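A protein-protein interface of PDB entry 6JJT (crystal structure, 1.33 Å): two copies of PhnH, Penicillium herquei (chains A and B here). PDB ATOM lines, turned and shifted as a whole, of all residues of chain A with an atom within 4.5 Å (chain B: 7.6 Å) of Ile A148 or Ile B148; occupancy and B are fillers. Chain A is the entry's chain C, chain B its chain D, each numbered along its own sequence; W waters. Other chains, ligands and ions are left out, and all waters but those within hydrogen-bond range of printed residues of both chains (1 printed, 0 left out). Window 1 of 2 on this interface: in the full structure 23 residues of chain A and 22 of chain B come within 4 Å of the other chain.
O of Pro A24 touches CD1 of Leu B26 (3.6 Å).
Pro A24 touches Trp B146 (CD to CD1, 3.96 Å).
Leu A26 touches Leu B26.
Tyr B110 touches Thr A129.
Trp A131 touches Pro B24 (CZ3 to CB, 3.6 Å).
Trp A146 touches Pro B23.
Pro B24 touches Trp A146.
Trp B131 touches Ile A148.
Glu A149 touches Tyr B110 (CB to CZ, 3.5 Å).
Glu A149 touches Trp B131 (CA to CZ2, 3.9 Å).
Of the 20 printed residues of chain B, 9 touch a printed residue of chain A.
Hydrophobic or aromatic side chains of chain A within 4 Å of the printed part of chain B: Pro A24, Leu A26, Trp A131, Trp A146 and Ile A148.
Among the printed residues, 17 pairs touch across the chains.
Among the printed residues, no Asp or Glu carboxylate lies within 4 Å of a Lys or Arg side-chain nitrogen of the other chain.
Water W1 bridges OH of Tyr B110 (2.7 Å) and OXT of Glu A149 (3.5 Å).
Of the printed residues of chain B, Pro A24 touches Leu B26 (3.6 Å), Trp B131 (3.6 Å) and Trp B146 (3.96 Å).
Of the printed residues of chain B, Trp A146 touches Pro B23 (3.4 Å) and Pro B24 (3.997 Å).
Ile A148 touches two residues of chain B.
Printed residues of chain A within 4 Å of Pro B23: Trp A146 (3.4 Å).
The nearest printed residue of chain A that does not touch Ile B148 is Leu A26 (5.0 Å).
N of Asn B25 is in hydrogen-bond range of O of Glu B149, at 2.8 Å.
The backbone carbonyl oxygen (O) of Trp B131 lies within hydrogen-bond range of the backbone NH (N) of Trp B146, at 2.7 Å.
The side-chain amide nitrogen (NE2) of Gln A147 is in hydrogen-bond range of the side-chain carboxylate (OE1) of Glu A149, 2.9 Å away.
N of Ile A148 lies within hydrogen-bond range of O of Thr A129 (3.0 Å).
The backbone NH of Trp A146 sits at hydrogen-bond distance from the backbone carbonyl oxygen of Trp A131, at 2.7 Å.
The backbone NH (N) of Ile B148 sits at hydrogen-bond distance from the backbone carbonyl oxygen (O) of Thr B129 (3.0 Å).
Pro A24 touches Leu B26, and with the chains exchanged Leu A26 touches Pro B24.
Pro A24 touches Trp B146, and with the chains exchanged Trp A146 touches Pro B24.
Thr A129 touches Trp B131, and with the chains exchanged Trp A131 touches Thr B129.
Ile A148 touches its own counterpart, Ile B148.
Of the 17 pairs that touch across the chains among the printed residues, 14 have their exchanged pair printed and touching as well.
OG1 of Thr A129 lies within hydrogen-bond range of NE1 of Trp B131, at 2.9 Å.
NE1 of Trp A131 sits at hydrogen-bond distance from OG1 of Thr B129 (2.8 Å).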
ATOM      1  N   PRO A  24     -15.312  -3.648   4.446  1.00  0.00           N
ATOM      2  CA  PRO A  24     -16.553  -3.489   3.662  1.00  0.00           C
ATOM      3  C   PRO A  24     -16.969  -4.868   3.149  1.00  0.00           C
ATOM      4  O   PRO A  24     -16.183  -5.798   3.218  1.00  0.00           O
ATOM      5  CB  PRO A  24     -16.062  -2.639   2.464  1.00  0.00           C
ATOM      6  CG  PRO A  24     -14.618  -3.065   2.317  1.00  0.00           C
ATOM      7  CD  PRO A  24     -14.105  -3.155   3.742  1.00  0.00           C
ATOM      8  N   ASN A  25     -18.193  -4.973   2.645  1.00  0.00           N
ATOM      9  CA  ASN A  25     -18.635  -6.209   2.028  1.00  0.00           C
ATOM     10  C   ASN A  25     -18.527  -6.092   0.510  1.00  0.00           C
ATOM     11  O   ASN A  25     -18.510  -4.986  -0.036  1.00  0.00           O
ATOM     12  CB  ASN A  25     -20.066  -6.527   2.418  1.00  0.00           C
ATOM     13  CG  ASN A  25     -20.144  -6.865   3.883  1.00  0.00           C
ATOM     14  OD1 ASN A  25     -19.541  -7.843   4.332  1.00  0.00           O
ATOM     15  ND2 ASN A  25     -20.840  -6.029   4.630  1.00  0.00           N
ATOM     16  N   LEU A  26     -18.438  -7.236  -0.157  1.00  0.00           N
ATOM     17  CA  LEU A  26     -18.251  -7.361  -1.596  1.00  0.00           C
ATOM     18  C   LEU A  26     -19.419  -8.137  -2.185  1.00  0.00           C
ATOM     19  O   LEU A  26     -19.772  -9.216  -1.666  1.00  0.00           O
ATOM     20  CB  LEU A  26     -16.918  -8.051  -1.890  1.00  0.00           C
ATOM     21  CG  LEU A  26     -15.731  -7.087  -2.086  1.00  0.00           C
ATOM     22  CD1 LEU A  26     -15.277  -6.512  -0.763  1.00  0.00           C
ATOM     23  CD2 LEU A  26     -14.557  -7.751  -2.779  1.00  0.00           C
ATOM     24  N   THR A 129     -18.082   2.181  -5.866  1.00  0.00           N
ATOM     25  CA  THR A 129     -16.699   1.821  -6.106  1.00  0.00           C
ATOM     26  C   THR A 129     -16.614   0.327  -6.382  1.00  0.00           C
ATOM     27  O   THR A 129     -17.139  -0.480  -5.565  1.00  0.00           O
ATOM     28  CB  THR A 129     -15.773   2.125  -4.927  1.00  0.00           C
ATOM     29  OG1 THR A 129     -16.467   1.681  -3.738  1.00  0.00           O
ATOM     30  CG2 THR A 129     -15.568   3.604  -4.722  1.00  0.00           C
ATOM     31  N   TRP A 131     -14.250  -3.198  -8.095  1.00  0.00           N
ATOM     32  CA  TRP A 131     -12.903  -3.734  -8.158  1.00  0.00           C
ATOM     33  C   TRP A 131     -12.944  -5.026  -8.972  1.00  0.00           C
ATOM     34  O   TRP A 131     -13.883  -5.839  -8.780  1.00  0.00           O
ATOM     35  CB  TRP A 131     -12.362  -4.027  -6.745  1.00  0.00           C
ATOM     36  CG  TRP A 131     -10.946  -4.501  -6.662  1.00  0.00           C
ATOM     37  CD1 TRP A 131      -9.819  -3.755  -6.403  1.00  0.00           C
ATOM     38  CD2 TRP A 131     -10.462  -5.858  -6.891  1.00  0.00           C
ATOM     39  NE1 TRP A 131      -8.679  -4.515  -6.425  1.00  0.00           N
ATOM     40  CE2 TRP A 131      -9.061  -5.826  -6.710  1.00  0.00           C
ATOM     41  CE3 TRP A 131     -11.063  -7.118  -7.169  1.00  0.00           C
ATOM     42  CZ2 TRP A 131      -8.266  -6.969  -6.829  1.00  0.00           C
ATOM     43  CZ3 TRP A 131     -10.263  -8.234  -7.353  1.00  0.00           C
ATOM     44  CH2 TRP A 131      -8.896  -8.164  -7.126  1.00  0.00           C
ATOM     45  N   TRP A 146     -16.525  -6.587  -8.673  1.00  0.00           N
ATOM     46  CA  TRP A 146     -17.224  -6.641  -7.390  1.00  0.00           C
ATOM     47  C   TRP A 146     -17.490  -5.233  -6.891  1.00  0.00           C
ATOM     48  O   TRP A 146     -16.582  -4.386  -6.974  1.00  0.00           O
ATOM     49  CB  TRP A 146     -16.336  -7.330  -6.318  1.00  0.00           C
ATOM     50  CG  TRP A 146     -16.013  -8.730  -6.719  1.00  0.00           C
ATOM     51  CD1 TRP A 146     -15.057  -9.115  -7.619  1.00  0.00           C
ATOM     52  CD2 TRP A 146     -16.761  -9.890  -6.325  1.00  0.00           C
ATOM     53  NE1 TRP A 146     -15.150 -10.480  -7.772  1.00  0.00           N
ATOM     54  CE2 TRP A 146     -16.206 -10.969  -7.037  1.00  0.00           C
ATOM     55  CE3 TRP A 146     -17.838 -10.091  -5.461  1.00  0.00           C
ATOM     56  CZ2 TRP A 146     -16.683 -12.285  -6.847  1.00  0.00           C
ATOM     57  CZ3 TRP A 146     -18.319 -11.388  -5.282  1.00  0.00           C
ATOM     58  CH2 TRP A 146     -17.753 -12.447  -5.991  1.00  0.00           C
ATOM     59  N   GLN A 147     -18.702  -4.977  -6.440  1.00  0.00           N
ATOM     60  CA  GLN A 147     -19.093  -3.757  -5.752  1.00  0.00           C
ATOM     61  C   GLN A 147     -18.573  -3.836  -4.323  1.00  0.00           C
ATOM     62  O   GLN A 147     -18.915  -4.782  -3.594  1.00  0.00           O
ATOM     63  CB  GLN A 147     -20.624  -3.653  -5.793  1.00  0.00           C
ATOM     64  CG  GLN A 147     -21.217  -2.494  -4.987  1.00  0.00           C
ATOM     65  CD  GLN A 147     -22.631  -2.137  -5.369  1.00  0.00           C
ATOM     66  OE1 GLN A 147     -23.175  -2.629  -6.366  1.00  0.00           O
ATOM     67  NE2 GLN A 147     -23.248  -1.217  -4.642  1.00  0.00           N
ATOM     68  N   ILE A 148     -17.842  -2.830  -3.854  1.00  0.00           N
ATOM     69  CA  ILE A 148     -17.297  -2.802  -2.496  1.00  0.00           C
ATOM     70  C   ILE A 148     -17.958  -1.664  -1.726  1.00  0.00           C
ATOM     71  O   ILE A 148     -17.895  -0.507  -2.161  1.00  0.00           O
ATOM     72  CB  ILE A 148     -15.788  -2.535  -2.532  1.00  0.00           C
ATOM     73  CG1 ILE A 148     -15.043  -3.484  -3.456  1.00  0.00           C
ATOM     74  CG2 ILE A 148     -15.191  -2.544  -1.134  1.00  0.00           C
ATOM     75  CD1 ILE A 148     -13.613  -3.039  -3.615  1.00  0.00           C
ATOM     76  N   GLU A 149     -18.553  -1.948  -0.562  1.00  0.00           N
ATOM     77  CA  GLU A 149     -19.054  -0.914   0.326  1.00  0.00           C
ATOM     78  C   GLU A 149     -19.489  -1.527   1.660  1.00  0.00           C
ATOM     79  O   GLU A 149     -19.607  -2.752   1.730  1.00  0.00           O
ATOM     80  CB  GLU A 149     -20.207  -0.130  -0.295  1.00  0.00           C
ATOM     81  CG  GLU A 149     -21.394  -0.953  -0.735  1.00  0.00           C
ATOM     82  CD  GLU A 149     -22.424  -0.037  -1.377  1.00  0.00           C
ATOM     83  OE1 GLU A 149     -22.185   0.460  -2.504  1.00  0.00           O
ATOM     84  OE2 GLU A 149     -23.467   0.219  -0.738  1.00  0.00           O
ATOM     85  OXT GLU A 149     -19.704  -0.723   2.597  1.00  0.00           O
ATOM     86  N   PRO B  23     -14.634 -13.789  -4.646  1.00  0.00           N
ATOM     87  CA  PRO B  23     -14.130 -12.454  -4.318  1.00  0.00           C
ATOM     88  C   PRO B  23     -12.655 -12.444  -3.938  1.00  0.00           C
ATOM     89  O   PRO B  23     -12.027 -13.443  -3.565  1.00  0.00           O
ATOM     90  CB  PRO B  23     -15.017 -12.005  -3.159  1.00  0.00           C
ATOM     91  CG  PRO B  23     -15.360 -13.316  -2.447  1.00  0.00           C
ATOM     92  CD  PRO B  23     -15.472 -14.339  -3.566  1.00  0.00           C
ATOM     93  N   PRO B  24     -12.016 -11.254  -4.007  1.00  0.00           N
ATOM     94  CA  PRO B  24     -10.659 -11.074  -3.512  1.00  0.00           C
ATOM     95  C   PRO B  24     -10.671 -11.089  -1.980  1.00  0.00           C
ATOM     96  O   PRO B  24     -11.729 -11.061  -1.361  1.00  0.00           O
ATOM     97  CB  PRO B  24     -10.340  -9.652  -4.024  1.00  0.00           C
ATOM     98  CG  PRO B  24     -11.661  -8.978  -4.038  1.00  0.00           C
ATOM     99  CD  PRO B  24     -12.584 -10.031  -4.616  1.00  0.00           C
ATOM    100  N   ASN B  25      -9.472 -11.061  -1.410  1.00  0.00           N
ATOM    101  CA  ASN B  25      -9.299 -10.949   0.032  1.00  0.00           C
ATOM    102  C   ASN B  25      -9.047  -9.484   0.392  1.00  0.00           C
ATOM    103  O   ASN B  25      -8.496  -8.750  -0.452  1.00  0.00           O
ATOM    104  CB  ASN B  25      -8.137 -11.824   0.526  1.00  0.00           C
ATOM    105  CG  ASN B  25      -8.392 -13.306   0.325  1.00  0.00           C
ATOM    106  OD1 ASN B  25      -7.637 -13.969  -0.385  1.00  0.00           O
ATOM    107  ND2 ASN B  25      -9.471 -13.814   0.901  1.00  0.00           N
ATOM    108  N   LEU B  26      -9.440  -9.104   1.621  1.00  0.00           N
ATOM    109  CA  LEU B  26      -9.270  -7.766   2.203  1.00  0.00           C
ATOM    110  C   LEU B  26      -8.359  -7.881   3.428  1.00  0.00           C
ATOM    111  O   LEU B  26      -8.583  -8.742   4.288  1.00  0.00           O
ATOM    112  CB  LEU B  26     -10.623  -7.198   2.630  1.00  0.00           C
ATOM    113  CG  LEU B  26     -11.646  -6.994   1.516  1.00  0.00           C
ATOM    114  CD1 LEU B  26     -13.062  -7.104   2.064  1.00  0.00           C
ATOM    115  CD2 LEU B  26     -11.467  -5.627   0.901  1.00  0.00           C
ATOM    116  N   GLU B  27      -7.347  -7.010   3.532  1.00  0.00           N
ATOM    117  CA  GLU B  27      -6.452  -6.961   4.679  1.00  0.00           C
ATOM    118  C   GLU B  27      -6.305  -5.509   5.106  1.00  0.00           C
ATOM    119  O   GLU B  27      -6.158  -4.631   4.262  1.00  0.00           O
ATOM    120  CB  GLU B  27      -5.078  -7.522   4.310  1.00  0.00           C
ATOM    121  CG  GLU B  27      -4.953  -9.040   4.394  1.00  0.00           C
ATOM    122  CD  GLU B  27      -5.606  -9.695   5.609  1.00  0.00           C
ATOM    123  OE1 GLU B  27      -5.314  -9.275   6.767  1.00  0.00           O
ATOM    124  OE2 GLU B  27      -6.439 -10.613   5.402  1.00  0.00           O
ATOM    125  N   LEU B  29      -4.884  -2.089   5.853  1.00  0.00           N
ATOM    126  CA  LEU B  29      -3.645  -1.524   5.339  1.00  0.00           C
ATOM    127  C   LEU B  29      -3.167  -0.331   6.168  1.00  0.00           C
ATOM    128  O   LEU B  29      -1.986  -0.312   6.496  1.00  0.00           O
ATOM    129  CB  LEU B  29      -3.842  -1.105   3.869  1.00  0.00           C
ATOM    130  CG  LEU B  29      -2.596  -0.644   3.110  1.00  0.00           C
ATOM    131  CD1 LEU B  29      -1.513  -1.703   3.018  1.00  0.00           C
ATOM    132  CD2 LEU B  29      -2.960  -0.087   1.729  1.00  0.00           C
ATOM    133  N   TYR B 110     -16.910   6.384  -0.244  1.00  0.00           N
ATOM    134  CA  TYR B 110     -16.045   5.261  -0.563  1.00  0.00           C
ATOM    135  C   TYR B 110     -14.840   5.717  -1.410  1.00  0.00           C
ATOM    136  O   TYR B 110     -15.041   6.365  -2.479  1.00  0.00           O
ATOM    137  CB  TYR B 110     -16.861   4.257  -1.384  1.00  0.00           C
ATOM    138  CG  TYR B 110     -18.189   3.893  -0.735  1.00  0.00           C
ATOM    139  CD1 TYR B 110     -18.280   3.640   0.651  1.00  0.00           C
ATOM    140  CD2 TYR B 110     -19.364   3.842  -1.465  1.00  0.00           C
ATOM    141  CE1 TYR B 110     -19.491   3.334   1.262  1.00  0.00           C
ATOM    142  CE2 TYR B 110     -20.579   3.559  -0.861  1.00  0.00           C
ATOM    143  CZ  TYR B 110     -20.638   3.289   0.493  1.00  0.00           C
ATOM    144  OH  TYR B 110     -21.855   2.977   1.064  1.00  0.00           O
ATOM    145  N   VAL B 111     -13.649   5.347  -0.977  1.00  0.00           N
ATOM    146  CA  VAL B 111     -12.410   5.903  -1.515  1.00  0.00           C
ATOM    147  C   VAL B 111     -11.525   4.795  -2.043  1.00  0.00           C
ATOM    148  O   VAL B 111     -11.122   3.903  -1.304  1.00  0.00           O
ATOM    149  CB  VAL B 111     -11.667   6.718  -0.437  1.00  0.00           C
ATOM    150  CG1 VAL B 111     -10.420   7.384  -1.048  1.00  0.00           C
ATOM    151  CG2 VAL B 111     -12.589   7.745   0.203  1.00  0.00           C
ATOM    152  N   ALA B 112     -11.142   4.881  -3.319  1.00  0.00           N
ATOM    153  CA  ALA B 112     -10.181   3.946  -3.888  1.00  0.00           C
ATOM    154  C   ALA B 112      -8.811   4.604  -3.897  1.00  0.00           C
ATOM    155  O   ALA B 112      -8.742   5.830  -4.154  1.00  0.00           O
ATOM    156  CB  ALA B 112     -10.580   3.617  -5.318  1.00  0.00           C
ATOM    157  N   ASN B 127       2.108  -2.082  -6.262  1.00  0.00           N
ATOM    158  CA  ASN B 127       1.249  -3.123  -6.789  1.00  0.00           C
ATOM    159  C   ASN B 127      -0.064  -3.234  -6.044  1.00  0.00           C
ATOM    160  O   ASN B 127      -0.799  -4.193  -6.281  1.00  0.00           O
ATOM    161  CB  ASN B 127       1.970  -4.477  -6.780  1.00  0.00           C
ATOM    162  CG  ASN B 127       3.201  -4.430  -7.647  1.00  0.00           C
ATOM    163  OD1 ASN B 127       3.159  -3.932  -8.771  1.00  0.00           O
ATOM    164  ND2 ASN B 127       4.330  -4.843  -7.092  1.00  0.00           N
ATOM    165  N   VAL B 128      -0.400  -2.285  -5.171  1.00  0.00           N
ATOM    166  CA  VAL B 128      -1.578  -2.371  -4.333  1.00  0.00           C
ATOM    167  C   VAL B 128      -2.738  -1.507  -4.833  1.00  0.00           C
ATOM    168  O   VAL B 128      -2.572  -0.305  -5.120  1.00  0.00           O
ATOM    169  CB  VAL B 128      -1.258  -1.977  -2.867  1.00  0.00           C
ATOM    170  CG1 VAL B 128      -2.504  -1.849  -2.000  1.00  0.00           C
ATOM    171  CG2 VAL B 128      -0.237  -2.978  -2.284  1.00  0.00           C
ATOM    172  N   THR B 129      -3.940  -2.061  -4.847  1.00  0.00           N
ATOM    173  CA  THR B 129      -5.179  -1.296  -4.884  1.00  0.00           C
ATOM    174  C   THR B 129      -5.787  -1.333  -3.489  1.00  0.00           C
ATOM    175  O   THR B 129      -6.076  -2.446  -2.929  1.00  0.00           O
ATOM    176  CB  THR B 129      -6.236  -1.925  -5.810  1.00  0.00           C
ATOM    177  OG1 THR B 129      -6.248  -3.364  -5.592  1.00  0.00           O
ATOM    178  CG2 THR B 129      -5.874  -1.760  -7.262  1.00  0.00           C
ATOM    179  N   ALA B 130      -6.025  -0.177  -2.885  1.00  0.00           N
ATOM    180  CA  ALA B 130      -6.713  -0.109  -1.606  1.00  0.00           C
ATOM    181  C   ALA B 130      -8.044   0.592  -1.677  1.00  0.00           C
ATOM    182  O   ALA B 130      -8.390   1.236  -2.680  1.00  0.00           O
ATOM    183  CB  ALA B 130      -5.795   0.521  -0.575  1.00  0.00           C
ATOM    184  N   TRP B 131      -8.800   0.543  -0.575  1.00  0.00           N
ATOM    185  CA  TRP B 131     -10.151   1.057  -0.498  1.00  0.00           C
ATOM    186  C   TRP B 131     -10.391   1.486   0.943  1.00  0.00           C
ATOM    187  O   TRP B 131      -9.996   0.719   1.845  1.00  0.00           O
ATOM    188  CB  TRP B 131     -11.154  -0.040  -0.881  1.00  0.00           C
ATOM    189  CG  TRP B 131     -12.567   0.411  -0.890  1.00  0.00           C
ATOM    190  CD1 TRP B 131     -13.309   0.793  -1.979  1.00  0.00           C
ATOM    191  CD2 TRP B 131     -13.472   0.535   0.222  1.00  0.00           C
ATOM    192  NE1 TRP B 131     -14.569   1.140  -1.631  1.00  0.00           N
ATOM    193  CE2 TRP B 131     -14.713   0.977  -0.283  1.00  0.00           C
ATOM    194  CE3 TRP B 131     -13.369   0.298   1.607  1.00  0.00           C
ATOM    195  CZ2 TRP B 131     -15.818   1.238   0.508  1.00  0.00           C
ATOM    196  CZ3 TRP B 131     -14.472   0.551   2.396  1.00  0.00           C
ATOM    197  CH2 TRP B 131     -15.685   0.974   1.856  1.00  0.00           C
ATOM    198  N   GLY B 132     -11.011   2.649   1.139  1.00  0.00           N
ATOM    199  CA  GLY B 132     -11.240   3.129   2.494  1.00  0.00           C
ATOM    200  C   GLY B 132     -12.532   3.887   2.623  1.00  0.00           C
ATOM    201  O   GLY B 132     -13.154   4.277   1.640  1.00  0.00           O
ATOM    202  N   TYR B 145      -8.403   2.069   5.720  1.00  0.00           N
ATOM    203  CA  TYR B 145      -8.180   1.544   4.370  1.00  0.00           C
ATOM    204  C   TYR B 145      -7.738   0.089   4.386  1.00  0.00           C
ATOM    205  O   TYR B 145      -6.940  -0.326   5.240  1.00  0.00           O
ATOM    206  CB  TYR B 145      -7.100   2.365   3.656  1.00  0.00           C
ATOM    207  CG  TYR B 145      -7.398   3.824   3.427  1.00  0.00           C
ATOM    208  CD1 TYR B 145      -7.068   4.742   4.406  1.00  0.00           C
ATOM    209  CD2 TYR B 145      -7.971   4.292   2.239  1.00  0.00           C
ATOM    210  CE1 TYR B 145      -7.305   6.101   4.230  1.00  0.00           C
ATOM    211  CE2 TYR B 145      -8.211   5.656   2.055  1.00  0.00           C
ATOM    212  CZ  TYR B 145      -7.883   6.550   3.058  1.00  0.00           C
ATOM    213  OH  TYR B 145      -8.051   7.910   2.891  1.00  0.00           O
ATOM    214  N   TRP B 146      -8.159  -0.642   3.336  1.00  0.00           N
ATOM    215  CA  TRP B 146      -7.952  -2.072   3.146  1.00  0.00           C
ATOM    216  C   TRP B 146      -7.235  -2.330   1.831  1.00  0.00           C
ATOM    217  O   TRP B 146      -7.625  -1.755   0.802  1.00  0.00           O
ATOM    218  CB  TRP B 146      -9.319  -2.771   3.151  1.00  0.00           C
ATOM    219  CG  TRP B 146     -10.000  -2.574   4.470  1.00  0.00           C
ATOM    220  CD1 TRP B 146     -10.700  -1.471   4.870  1.00  0.00           C
ATOM    221  CD2 TRP B 146      -9.974  -3.473   5.586  1.00  0.00           C
ATOM    222  NE1 TRP B 146     -11.139  -1.634   6.161  1.00  0.00           N
ATOM    223  CE2 TRP B 146     -10.688  -2.843   6.631  1.00  0.00           C
ATOM    224  CE3 TRP B 146      -9.433  -4.743   5.779  1.00  0.00           C
ATOM    225  CZ2 TRP B 146     -10.903  -3.473   7.860  1.00  0.00           C
ATOM    226  CZ3 TRP B 146      -9.620  -5.354   7.002  1.00  0.00           C
ATOM    227  CH2 TRP B 146     -10.336  -4.718   8.017  1.00  0.00           C
ATOM    228  N   GLN B 147      -6.274  -3.252   1.807  1.00  0.00           N
ATOM    229  CA  GLN B 147      -5.670  -3.808   0.610  1.00  0.00           C
ATOM    230  C   GLN B 147      -6.615  -4.858   0.027  1.00  0.00           C
ATOM    231  O   GLN B 147      -7.106  -5.727   0.761  1.00  0.00           O
ATOM    232  CB  GLN B 147      -4.335  -4.463   0.961  1.00  0.00           C
ATOM    233  CG  GLN B 147      -3.568  -5.197  -0.136  1.00  0.00           C
ATOM    234  CD  GLN B 147      -2.164  -5.536   0.321  1.00  0.00           C
ATOM    235  OE1 GLN B 147      -1.820  -5.291   1.472  1.00  0.00           O
ATOM    236  NE2 GLN B 147      -1.339  -6.116  -0.534  1.00  0.00           N
ATOM    237  N   ILE B 148      -6.915  -4.744  -1.274  1.00  0.00           N
ATOM    238  CA  ILE B 148      -7.834  -5.668  -1.940  1.00  0.00           C
ATOM    239  C   ILE B 148      -7.013  -6.461  -2.924  1.00  0.00           C
ATOM    240  O   ILE B 148      -6.423  -5.859  -3.800  1.00  0.00           O
ATOM    241  CB  ILE B 148      -8.949  -4.934  -2.710  1.00  0.00           C
ATOM    242  CG1 ILE B 148      -9.679  -3.945  -1.821  1.00  0.00           C
ATOM    243  CG2 ILE B 148      -9.940  -5.933  -3.308  1.00  0.00           C
ATOM    244  CD1 ILE B 148     -10.710  -3.131  -2.561  1.00  0.00           C
ATOM    245  N   GLU B 149      -6.943  -7.796  -2.813  1.00  0.00           N
ATOM    246  CA  GLU B 149      -6.290  -8.607  -3.833  1.00  0.00           C
ATOM    247  C   GLU B 149      -6.572 -10.086  -3.601  1.00  0.00           C
ATOM    248  O   GLU B 149      -6.991 -10.400  -2.511  1.00  0.00           O
ATOM    249  CB  GLU B 149      -4.770  -8.445  -3.916  1.00  0.00           C
ATOM    250  CG  GLU B 149      -4.054  -8.557  -2.604  1.00  0.00           C
ATOM    251  CD  GLU B 149      -2.582  -8.204  -2.736  1.00  0.00           C
ATOM    252  OE1 GLU B 149      -2.230  -6.979  -2.952  1.00  0.00           O
ATOM    253  OE2 GLU B 149      -1.767  -9.155  -2.654  1.00  0.00           O
ATOM    254  OXT GLU B 149      -6.310 -10.846  -4.528  1.00  0.00           O
HETATM  255  O   HOH W   1     -21.913   1.781   3.470  1.00  0.00           O
